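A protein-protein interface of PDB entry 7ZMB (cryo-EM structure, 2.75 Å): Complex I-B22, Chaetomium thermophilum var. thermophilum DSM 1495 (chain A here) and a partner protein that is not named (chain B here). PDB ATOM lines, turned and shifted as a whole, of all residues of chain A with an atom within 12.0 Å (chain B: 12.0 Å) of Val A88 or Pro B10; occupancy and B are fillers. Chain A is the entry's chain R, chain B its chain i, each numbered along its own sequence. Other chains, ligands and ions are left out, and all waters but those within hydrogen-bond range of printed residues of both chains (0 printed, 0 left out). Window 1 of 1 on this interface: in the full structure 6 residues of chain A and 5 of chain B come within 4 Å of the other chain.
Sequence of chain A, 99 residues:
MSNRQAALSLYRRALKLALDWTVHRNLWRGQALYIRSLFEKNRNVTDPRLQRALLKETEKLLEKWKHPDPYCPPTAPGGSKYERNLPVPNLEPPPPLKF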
ATOM      1  N   GLU A  83      26.971  -1.729  25.597  1.00  0.00           N
ATOM      2  CA  GLU A  83      25.716  -1.084  25.988  1.00  0.00           C
ATOM      3  C   GLU A  83      25.807  -0.374  27.335  1.00  0.00           C
ATOM      4  O   GLU A  83      24.871  -0.432  28.132  1.00  0.00           O
ATOM      5  CB  GLU A  83      24.550  -2.095  25.975  1.00  0.00           C
ATOM      6  CG  GLU A  83      24.644  -3.278  26.931  1.00  0.00           C
ATOM      7  CD  GLU A  83      23.431  -4.184  26.874  1.00  0.00           C
ATOM      8  OE1 GLU A  83      22.569  -3.972  25.998  1.00  0.00           O
ATOM      9  OE2 GLU A  83      23.335  -5.102  27.711  1.00  0.00           O
ATOM     10  N   ARG A  84      26.910   0.344  27.571  1.00  0.00           N
ATOM     11  CA  ARG A  84      27.146   0.988  28.861  1.00  0.00           C
ATOM     12  C   ARG A  84      26.401   2.312  28.992  1.00  0.00           C
ATOM     13  O   ARG A  84      25.587   2.491  29.905  1.00  0.00           O
ATOM     14  CB  ARG A  84      28.641   1.219  29.069  1.00  0.00           C
ATOM     15  CG  ARG A  84      28.945   2.214  30.177  1.00  0.00           C
ATOM     16  CD  ARG A  84      30.419   2.314  30.447  1.00  0.00           C
ATOM     17  NE  ARG A  84      30.899   1.180  31.223  1.00  0.00           N
ATOM     18  CZ  ARG A  84      32.176   0.960  31.506  1.00  0.00           C
ATOM     19  NH1 ARG A  84      33.105   1.795  31.071  1.00  0.00           N
ATOM     20  NH2 ARG A  84      32.523  -0.098  32.219  1.00  0.00           N
ATOM     21  N   ASN A  85      26.692   3.261  28.106  1.00  0.00           N
ATOM     22  CA  ASN A  85      26.099   4.594  28.137  1.00  0.00           C
ATOM     23  C   ASN A  85      25.258   4.732  26.875  1.00  0.00           C
ATOM     24  O   ASN A  85      25.723   5.242  25.855  1.00  0.00           O
ATOM     25  CB  ASN A  85      27.171   5.669  28.218  1.00  0.00           C
ATOM     26  CG  ASN A  85      28.013   5.557  29.470  1.00  0.00           C
ATOM     27  OD1 ASN A  85      27.508   5.226  30.540  1.00  0.00           O
ATOM     28  ND2 ASN A  85      29.305   5.825  29.342  1.00  0.00           N
ATOM     29  N   LEU A  86      24.039   4.281  26.948  1.00  0.00           N
ATOM     30  CA  LEU A  86      23.226   4.213  25.747  1.00  0.00           C
ATOM     31  C   LEU A  86      22.395   5.477  25.596  1.00  0.00           C
ATOM     32  O   LEU A  86      21.674   5.850  26.528  1.00  0.00           O
ATOM     33  CB  LEU A  86      22.314   2.999  25.788  1.00  0.00           C
ATOM     34  CG  LEU A  86      23.033   1.658  25.688  1.00  0.00           C
ATOM     35  CD1 LEU A  86      22.033   0.512  25.680  1.00  0.00           C
ATOM     36  CD2 LEU A  86      23.902   1.626  24.444  1.00  0.00           C
ATOM     37  N   PRO A  87      22.472   6.158  24.458  1.00  0.00           N
ATOM     38  CA  PRO A  87      21.573   7.287  24.215  1.00  0.00           C
ATOM     39  C   PRO A  87      20.144   6.804  24.046  1.00  0.00           C
ATOM     40  O   PRO A  87      19.886   5.650  23.706  1.00  0.00           O
ATOM     41  CB  PRO A  87      22.111   7.899  22.919  1.00  0.00           C
ATOM     42  CG  PRO A  87      22.768   6.764  22.225  1.00  0.00           C
ATOM     43  CD  PRO A  87      23.336   5.878  23.299  1.00  0.00           C
ATOM     44  N   VAL A  88      19.208   7.703  24.301  1.00  0.00           N
ATOM     45  CA  VAL A  88      17.803   7.320  24.139  1.00  0.00           C
ATOM     46  C   VAL A  88      17.520   7.089  22.659  1.00  0.00           C
ATOM     47  O   VAL A  88      18.017   7.847  21.807  1.00  0.00           O
ATOM     48  CB  VAL A  88      16.881   8.389  24.729  1.00  0.00           C
ATOM     49  CG1 VAL A  88      17.342   8.764  26.127  1.00  0.00           C
ATOM     50  CG2 VAL A  88      16.777   9.595  23.824  1.00  0.00           C
ATOM     51  N   PRO A  89      16.801   6.032  22.299  1.00  0.00           N
ATOM     52  CA  PRO A  89      16.546   5.775  20.874  1.00  0.00           C
ATOM     53  C   PRO A  89      15.741   6.866  20.188  1.00  0.00           C
ATOM     54  O   PRO A  89      15.810   6.990  18.959  1.00  0.00           O
ATOM     55  CB  PRO A  89      15.787   4.443  20.894  1.00  0.00           C
ATOM     56  CG  PRO A  89      16.223   3.791  22.167  1.00  0.00           C
ATOM     57  CD  PRO A  89      16.414   4.900  23.151  1.00  0.00           C
ATOM     58  N   ASN A  90      14.984   7.658  20.940  1.00  0.00           N
ATOM     59  CA  ASN A  90      14.057   8.637  20.385  1.00  0.00           C
ATOM     60  C   ASN A  90      14.403  10.004  20.958  1.00  0.00           C
ATOM     61  O   ASN A  90      14.104  10.288  22.123  1.00  0.00           O
ATOM     62  CB  ASN A  90      12.617   8.239  20.708  1.00  0.00           C
ATOM     63  CG  ASN A  90      11.602   9.175  20.114  1.00  0.00           C
ATOM     64  OD1 ASN A  90      11.929  10.032  19.309  1.00  0.00           O
ATOM     65  ND2 ASN A  90      10.349   9.000  20.500  1.00  0.00           N
ATOM     66  N   LEU A  91      15.027  10.851  20.142  1.00  0.00           N
ATOM     67  CA  LEU A  91      15.450  12.169  20.595  1.00  0.00           C
ATOM     68  C   LEU A  91      14.371  13.231  20.475  1.00  0.00           C
ATOM     69  O   LEU A  91      14.524  14.305  21.065  1.00  0.00           O
ATOM     70  CB  LEU A  91      16.682  12.635  19.814  1.00  0.00           C
ATOM     71  CG  LEU A  91      18.066  12.157  20.258  1.00  0.00           C
ATOM     72  CD1 LEU A  91      18.374  12.688  21.650  1.00  0.00           C
ATOM     73  CD2 LEU A  91      18.185  10.643  20.220  1.00  0.00           C
ATOM     74  N   GLU A  92      13.305  12.975  19.732  1.00  0.00           N
ATOM     75  CA  GLU A  92      12.305  14.014  19.534  1.00  0.00           C
ATOM     76  C   GLU A  92      11.429  14.166  20.777  1.00  0.00           C
ATOM     77  O   GLU A  92      11.116  13.176  21.443  1.00  0.00           O
ATOM     78  CB  GLU A  92      11.447  13.705  18.313  1.00  0.00           C
ATOM     79  CG  GLU A  92      12.202  13.781  16.989  1.00  0.00           C
ATOM     80  CD  GLU A  92      12.980  12.523  16.663  1.00  0.00           C
ATOM     81  OE1 GLU A  92      12.893  11.549  17.434  1.00  0.00           O
ATOM     82  OE2 GLU A  92      13.675  12.505  15.625  1.00  0.00           O
ATOM     83  N   PRO A  93      11.023  15.396  21.106  1.00  0.00           N
ATOM     84  CA  PRO A  93      10.254  15.609  22.332  1.00  0.00           C
ATOM     85  C   PRO A  93       8.867  15.003  22.222  1.00  0.00           C
ATOM     86  O   PRO A  93       8.337  14.821  21.113  1.00  0.00           O
ATOM     87  CB  PRO A  93      10.186  17.143  22.446  1.00  0.00           C
ATOM     88  CG  PRO A  93      11.180  17.675  21.448  1.00  0.00           C
ATOM     89  CD  PRO A  93      11.270  16.650  20.376  1.00  0.00           C
ATOM     90  N   PRO A  94       8.240  14.664  23.351  1.00  0.00           N
ATOM     91  CA  PRO A  94       6.912  14.062  23.297  1.00  0.00           C
ATOM     92  C   PRO A  94       5.878  15.048  22.788  1.00  0.00           C
ATOM     93  O   PRO A  94       5.984  16.263  23.027  1.00  0.00           O
ATOM     94  CB  PRO A  94       6.643  13.674  24.763  1.00  0.00           C
ATOM     95  CG  PRO A  94       7.995  13.576  25.371  1.00  0.00           C
ATOM     96  CD  PRO A  94       8.784  14.660  24.717  1.00  0.00           C
ATOM     97  N   PRO A  95       4.841  14.568  22.108  1.00  0.00           N
ATOM     98  CA  PRO A  95       3.866  15.464  21.486  1.00  0.00           C
ATOM     99  C   PRO A  95       2.907  16.031  22.515  1.00  0.00           C
ATOM    100  O   PRO A  95       2.853  15.549  23.656  1.00  0.00           O
ATOM    101  CB  PRO A  95       3.139  14.537  20.503  1.00  0.00           C
ATOM    102  CG  PRO A  95       3.158  13.237  21.195  1.00  0.00           C
ATOM    103  CD  PRO A  95       4.492  13.156  21.890  1.00  0.00           C
ATOM    104  N   LYS B   6      30.682  13.320  23.309  1.00  0.00           N
ATOM    105  CA  LYS B   6      29.545  13.569  24.183  1.00  0.00           C
ATOM    106  C   LYS B   6      28.330  12.839  23.634  1.00  0.00           C
ATOM    107  O   LYS B   6      27.994  12.988  22.456  1.00  0.00           O
ATOM    108  CB  LYS B   6      29.256  15.069  24.302  1.00  0.00           C
ATOM    109  CG  LYS B   6      28.578  15.467  25.598  1.00  0.00           C
ATOM    110  CD  LYS B   6      28.763  16.945  25.886  1.00  0.00           C
ATOM    111  CE  LYS B   6      30.236  17.297  26.023  1.00  0.00           C
ATOM    112  NZ  LYS B   6      30.437  18.720  26.410  1.00  0.00           N
ATOM    113  N   ILE B   7      27.681  12.056  24.483  1.00  0.00           N
ATOM    114  CA  ILE B   7      26.519  11.274  24.047  1.00  0.00           C
ATOM    115  C   ILE B   7      25.338  12.210  23.816  1.00  0.00           C
ATOM    116  O   ILE B   7      25.037  13.044  24.686  1.00  0.00           O
ATOM    117  CB  ILE B   7      26.175  10.210  25.087  1.00  0.00           C
ATOM    118  CG1 ILE B   7      27.434   9.460  25.520  1.00  0.00           C
ATOM    119  CG2 ILE B   7      25.138   9.246  24.537  1.00  0.00           C
ATOM    120  CD1 ILE B   7      27.994   8.544  24.455  1.00  0.00           C
ATOM    121  N   PRO B   8      24.653  12.129  22.679  1.00  0.00           N
ATOM    122  CA  PRO B   8      23.425  12.909  22.511  1.00  0.00           C
ATOM    123  C   PRO B   8      22.345  12.424  23.463  1.00  0.00           C
ATOM    124  O   PRO B   8      22.298  11.252  23.841  1.00  0.00           O
ATOM    125  CB  PRO B   8      23.038  12.656  21.051  1.00  0.00           C
ATOM    126  CG  PRO B   8      23.655  11.344  20.730  1.00  0.00           C
ATOM    127  CD  PRO B   8      24.942  11.295  21.503  1.00  0.00           C
ATOM    128  N   TYR B   9      21.469  13.344  23.855  1.00  0.00           N
ATOM    129  CA  TYR B   9      20.438  13.037  24.833  1.00  0.00           C
ATOM    130  C   TYR B   9      19.312  14.044  24.682  1.00  0.00           C
ATOM    131  O   TYR B   9      19.531  15.147  24.166  1.00  0.00           O
ATOM    132  CB  TYR B   9      21.006  13.066  26.256  1.00  0.00           C
ATOM    133  CG  TYR B   9      21.642  14.374  26.622  1.00  0.00           C
ATOM    134  CD1 TYR B   9      20.889  15.407  27.154  1.00  0.00           C
ATOM    135  CD2 TYR B   9      22.998  14.578  26.443  1.00  0.00           C
ATOM    136  CE1 TYR B   9      21.467  16.595  27.492  1.00  0.00           C
ATOM    137  CE2 TYR B   9      23.580  15.773  26.776  1.00  0.00           C
ATOM    138  CZ  TYR B   9      22.810  16.775  27.305  1.00  0.00           C
ATOM    139  OH  TYR B   9      23.390  17.971  27.641  1.00  0.00           O
ATOM    140  N   PRO B  10      18.100  13.703  25.125  1.00  0.00           N
ATOM    141  CA  PRO B  10      16.982  14.643  25.010  1.00  0.00           C
ATOM    142  C   PRO B  10      17.187  15.873  25.872  1.00  0.00           C
ATOM    143  O   PRO B  10      17.837  15.829  26.917  1.00  0.00           O
ATOM    144  CB  PRO B  10      15.777  13.834  25.501  1.00  0.00           C
ATOM    145  CG  PRO B  10      16.232  12.438  25.593  1.00  0.00           C
ATOM    146  CD  PRO B  10      17.699  12.468  25.813  1.00  0.00           C
ATOM    147  N   LYS B  11      16.609  16.981  25.428  1.00  0.00           N
ATOM    148  CA  LYS B  11      16.703  18.234  26.159  1.00  0.00           C
ATOM    149  C   LYS B  11      15.444  18.546  26.951  1.00  0.00           C
ATOM    150  O   LYS B  11      15.397  19.568  27.641  1.00  0.00           O
ATOM    151  CB  LYS B  11      17.013  19.382  25.196  1.00  0.00           C
ATOM    152  CG  LYS B  11      18.342  19.220  24.476  1.00  0.00           C
ATOM    153  CD  LYS B  11      19.511  19.328  25.436  1.00  0.00           C
ATOM    154  CE  LYS B  11      20.835  19.242  24.697  1.00  0.00           C
ATOM    155  NZ  LYS B  11      21.998  19.302  25.624  1.00  0.00           N
ATOM    156  N   HIS B  12      14.434  17.690  26.883  1.00  0.00           N
ATOM    157  CA  HIS B  12      13.190  17.920  27.593  1.00  0.00           C
ATOM    158  C   HIS B  12      13.142  17.240  28.950  1.00  0.00           C
ATOM    159  O   HIS B  12      12.279  17.582  29.765  1.00  0.00           O
ATOM    160  CB  HIS B  12      12.014  17.442  26.750  1.00  0.00           C
ATOM    161  CG  HIS B  12      12.216  16.094  26.133  1.00  0.00           C
ATOM    162  ND1 HIS B  12      11.666  14.945  26.659  1.00  0.00           N
ATOM    163  CD2 HIS B  12      12.879  15.717  25.017  1.00  0.00           C
ATOM    164  CE1 HIS B  12      11.991  13.916  25.901  1.00  0.00           C
ATOM    165  NE2 HIS B  12      12.723  14.356  24.895  1.00  0.00           N
ATOM    166  N   VAL B  13      14.061  16.320  29.224  1.00  0.00           N
ATOM    167  CA  VAL B  13      13.952  15.422  30.365  1.00  0.00           C
ATOM    168  C   VAL B  13      14.470  16.157  31.599  1.00  0.00           C
ATOM    169  O   VAL B  13      15.673  16.297  31.801  1.00  0.00           O
ATOM    170  CB  VAL B  13      14.701  14.116  30.112  1.00  0.00           C
ATOM    171  CG1 VAL B  13      14.727  13.273  31.349  1.00  0.00           C
ATOM    172  CG2 VAL B  13      14.053  13.361  28.971  1.00  0.00           C
ATOM    173  N   TRP B  14      13.549  16.623  32.432  1.00  0.00           N
ATOM    174  CA  TRP B  14      13.906  17.296  33.673  1.00  0.00           C
ATOM    175  C   TRP B  14      14.312  16.259  34.711  1.00  0.00           C
ATOM    176  O   TRP B  14      13.559  15.325  34.993  1.00  0.00           O
ATOM    177  CB  TRP B  14      12.735  18.137  34.176  1.00  0.00           C
ATOM    178  CG  TRP B  14      13.097  19.126  35.241  1.00  0.00           C
ATOM    179  CD1 TRP B  14      13.350  20.447  35.067  1.00  0.00           C
ATOM    180  CD2 TRP B  14      13.220  18.878  36.646  1.00  0.00           C
ATOM    181  NE1 TRP B  14      13.641  21.040  36.266  1.00  0.00           N
ATOM    182  CE2 TRP B  14      13.564  20.097  37.255  1.00  0.00           C
ATOM    183  CE3 TRP B  14      13.077  17.742  37.450  1.00  0.00           C
ATOM    184  CZ2 TRP B  14      13.770  20.215  38.628  1.00  0.00           C
ATOM    185  CZ3 TRP B  14      13.285  17.860  38.809  1.00  0.00           C
ATOM    186  CH2 TRP B  14      13.627  19.085  39.384  1.00  0.00           C
ATOM    187  N   SER B  15      15.494  16.426  35.276  1.00  0.00           N
ATOM    188  CA  SER B  15      16.007  15.552  36.308  1.00  0.00           C
ATOM    189  C   SER B  15      16.197  16.324  37.605  1.00  0.00           C
ATOM    190  O   SER B  15      16.498  17.519  37.582  1.00  0.00           O
ATOM    191  CB  SER B  15      17.343  14.929  35.896  1.00  0.00           C
ATOM    192  OG  SER B  15      17.862  14.103  36.918  1.00  0.00           O
ATOM    193  N   PRO B  16      16.009  15.685  38.750  1.00  0.00           N
ATOM    194  CA  PRO B  16      16.296  16.367  40.012  1.00  0.00           C
ATOM    195  C   PRO B  16      17.781  16.343  40.306  1.00  0.00           C
ATOM    196  O   PRO B  16      18.321  17.247  40.947  1.00  0.00           O
ATOM    197  CB  PRO B  16      15.490  15.562  41.033  1.00  0.00           C
ATOM    198  CG  PRO B  16      15.447  14.200  40.455  1.00  0.00           C
ATOM    199  CD  PRO B  16      15.441  14.343  38.964  1.00  0.00           C
ATOM    200  N   GLY B  18      19.935  16.497  37.860  1.00  0.00           N
ATOM    201  CA  GLY B  18      20.590  17.392  36.935  1.00  0.00           C
ATOM    202  C   GLY B  18      20.443  17.068  35.469  1.00  0.00           C
ATOM    203  O   GLY B  18      20.288  17.976  34.645  1.00  0.00           O
ATOM    204  N   GLY B  19      20.476  15.794  35.119  1.00  0.00           N
ATOM    205  CA  GLY B  19      20.385  15.447  33.719  1.00  0.00           C
ATOM    206  C   GLY B  19      21.670  14.823  33.226  1.00  0.00           C
ATOM    207  O   GLY B  19      22.319  14.089  33.973  1.00  0.00           O
ATOM    208  N   TRP B  20      22.064  15.105  31.984  1.00  0.00           N
ATOM    209  CA  TRP B  20      23.194  14.377  31.424  1.00  0.00           C
ATOM    210  C   TRP B  20      24.528  15.021  31.774  1.00  0.00           C
ATOM    211  O   TRP B  20      25.324  14.427  32.497  1.00  0.00           O
ATOM    212  CB  TRP B  20      23.034  14.233  29.913  1.00  0.00           C
ATOM    213  CG  TRP B  20      22.277  13.024  29.580  1.00  0.00           C
ATOM    214  CD1 TRP B  20      22.777  11.831  29.177  1.00  0.00           C
ATOM    215  CD2 TRP B  20      20.864  12.864  29.666  1.00  0.00           C
ATOM    216  NE1 TRP B  20      21.759  10.934  28.984  1.00  0.00           N
ATOM    217  CE2 TRP B  20      20.572  11.546  29.279  1.00  0.00           C
ATOM    218  CE3 TRP B  20      19.815  13.715  30.020  1.00  0.00           C
ATOM    219  CZ2 TRP B  20      19.281  11.059  29.231  1.00  0.00           C
ATOM    220  CZ3 TRP B  20      18.537  13.231  29.974  1.00  0.00           C
ATOM    221  CH2 TRP B  20      18.276  11.917  29.579  1.00  0.00           C
ATOM    222  N   TYR B  21      24.777  16.242  31.322  1.00  0.00           N
ATOM    223  CA  TYR B  21      26.057  16.847  31.668  1.00  0.00           C
ATOM    224  C   TYR B  21      25.819  18.152  32.402  1.00  0.00           C
ATOM    225  O   TYR B  21      26.426  19.179  32.085  1.00  0.00           O
ATOM    226  CB  TYR B  21      26.911  17.056  30.420  1.00  0.00           C
ATOM    227  CG  TYR B  21      27.254  15.766  29.718  1.00  0.00           C
ATOM    228  CD1 TYR B  21      26.401  15.220  28.777  1.00  0.00           C
ATOM    229  CD2 TYR B  21      28.430  15.095  29.998  1.00  0.00           C
ATOM    230  CE1 TYR B  21      26.704  14.046  28.142  1.00  0.00           C
ATOM    231  CE2 TYR B  21      28.746  13.920  29.366  1.00  0.00           C
ATOM    232  CZ  TYR B  21      27.882  13.399  28.438  1.00  0.00           C
ATOM    233  OH  TYR B  21      28.194  12.222  27.802  1.00  0.00           O
ATOM    234  N   ALA B  22      24.940  18.105  33.393  1.00  0.00           N
ATOM    235  CA  ALA B  22      24.375  19.313  33.968  1.00  0.00           C
ATOM    236  C   ALA B  22      25.405  20.108  34.757  1.00  0.00           C
ATOM    237  O   ALA B  22      26.103  19.569  35.617  1.00  0.00           O
ATOM    238  CB  ALA B  22      23.203  18.957  34.869  1.00  0.00           C
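The backbone NH (N) of Ile B7 lies within hydrogen-bond range of the side-chain hydroxyl (OH) of Tyr B21 (3.4 Å).
The side-chain hydroxyl (OH) of Tyr B9 is in hydrogen-bond range of the side-chain amino group (NZ) of Lys B11, at 2.8 Å.
The side-chain amide oxygen of Asn A90 lies close to the side-chain carboxylate of Glu A92, 2.6 Å away.
Among the printed residues, pairs that only touch across the chains: Pro A87 with Ile B7 (3.7 Å), Pro A87 with Pro B8 (3.5 Å), Val A88 with Pro B10 (3.4 Å), Leu A91 with Tyr B9 (3.5 Å), Leu A91 with Pro B10 (3.6 Å), Glu A92 with His B12 (3.99 Å), Pro A93 with His B12 (3.8 Å) and Pro A94 with His B12 (3.5 Å).
Arg A84 touches none of the printed residues of chain B.
No residue of chain B comes within 4 Å of Leu A86.
Printed residues of chain B within 4 Å of Pro A87: Ile B7 and Pro B8.
Val A88 touches just one residue of chain B: Pro B10.
Leu A91 touches two residues of chain B.
Lys B6 touches none of the printed residues of chain A.
Of the printed residues of chain A, Ile B7 touches Pro A87 (3.7 Å).
Of chain A, only Leu A91 (3.5 Å) comes within 4 Å of Tyr B9.
Pro B10 touches just these residues of chain A: Val A88 (3.4 Å) and Leu A91 (3.6 Å).
No residue of chain A comes within 4 Å of Lys B11.
Of the printed residues of chain A, His B12 touches Glu A92 (3.99 Å), Pro A93 (3.8 Å) and Pro A94 (3.5 Å).
No residue of chain A comes within 4 Å of Val B13.
The nearest residue of chain A that does not touch Pro B10 is Asn A90 (4.6 Å).
Of the 13 printed residues of chain A, 6 touch a printed residue of chain B.
Hydrophobic or aromatic side chains of chain A that line the printed part of chain B: Pro A87, Val A88, Leu A91, Pro A93 and Pro A94.
Along chain A the printed residues that touch a printed residue of chain B span positions 87 to 94.
Printed residues of chain B that touch a printed residue of chain A: Ile B7, Pro B8, Tyr B9, Pro B10 and His B12.
Among the printed residues, 8 pairs touch across the chains.
Among the printed residues, no Asp or Glu carboxylate lies within 4 Å of a Lys or Arg side-chain nitrogen of the other chain.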
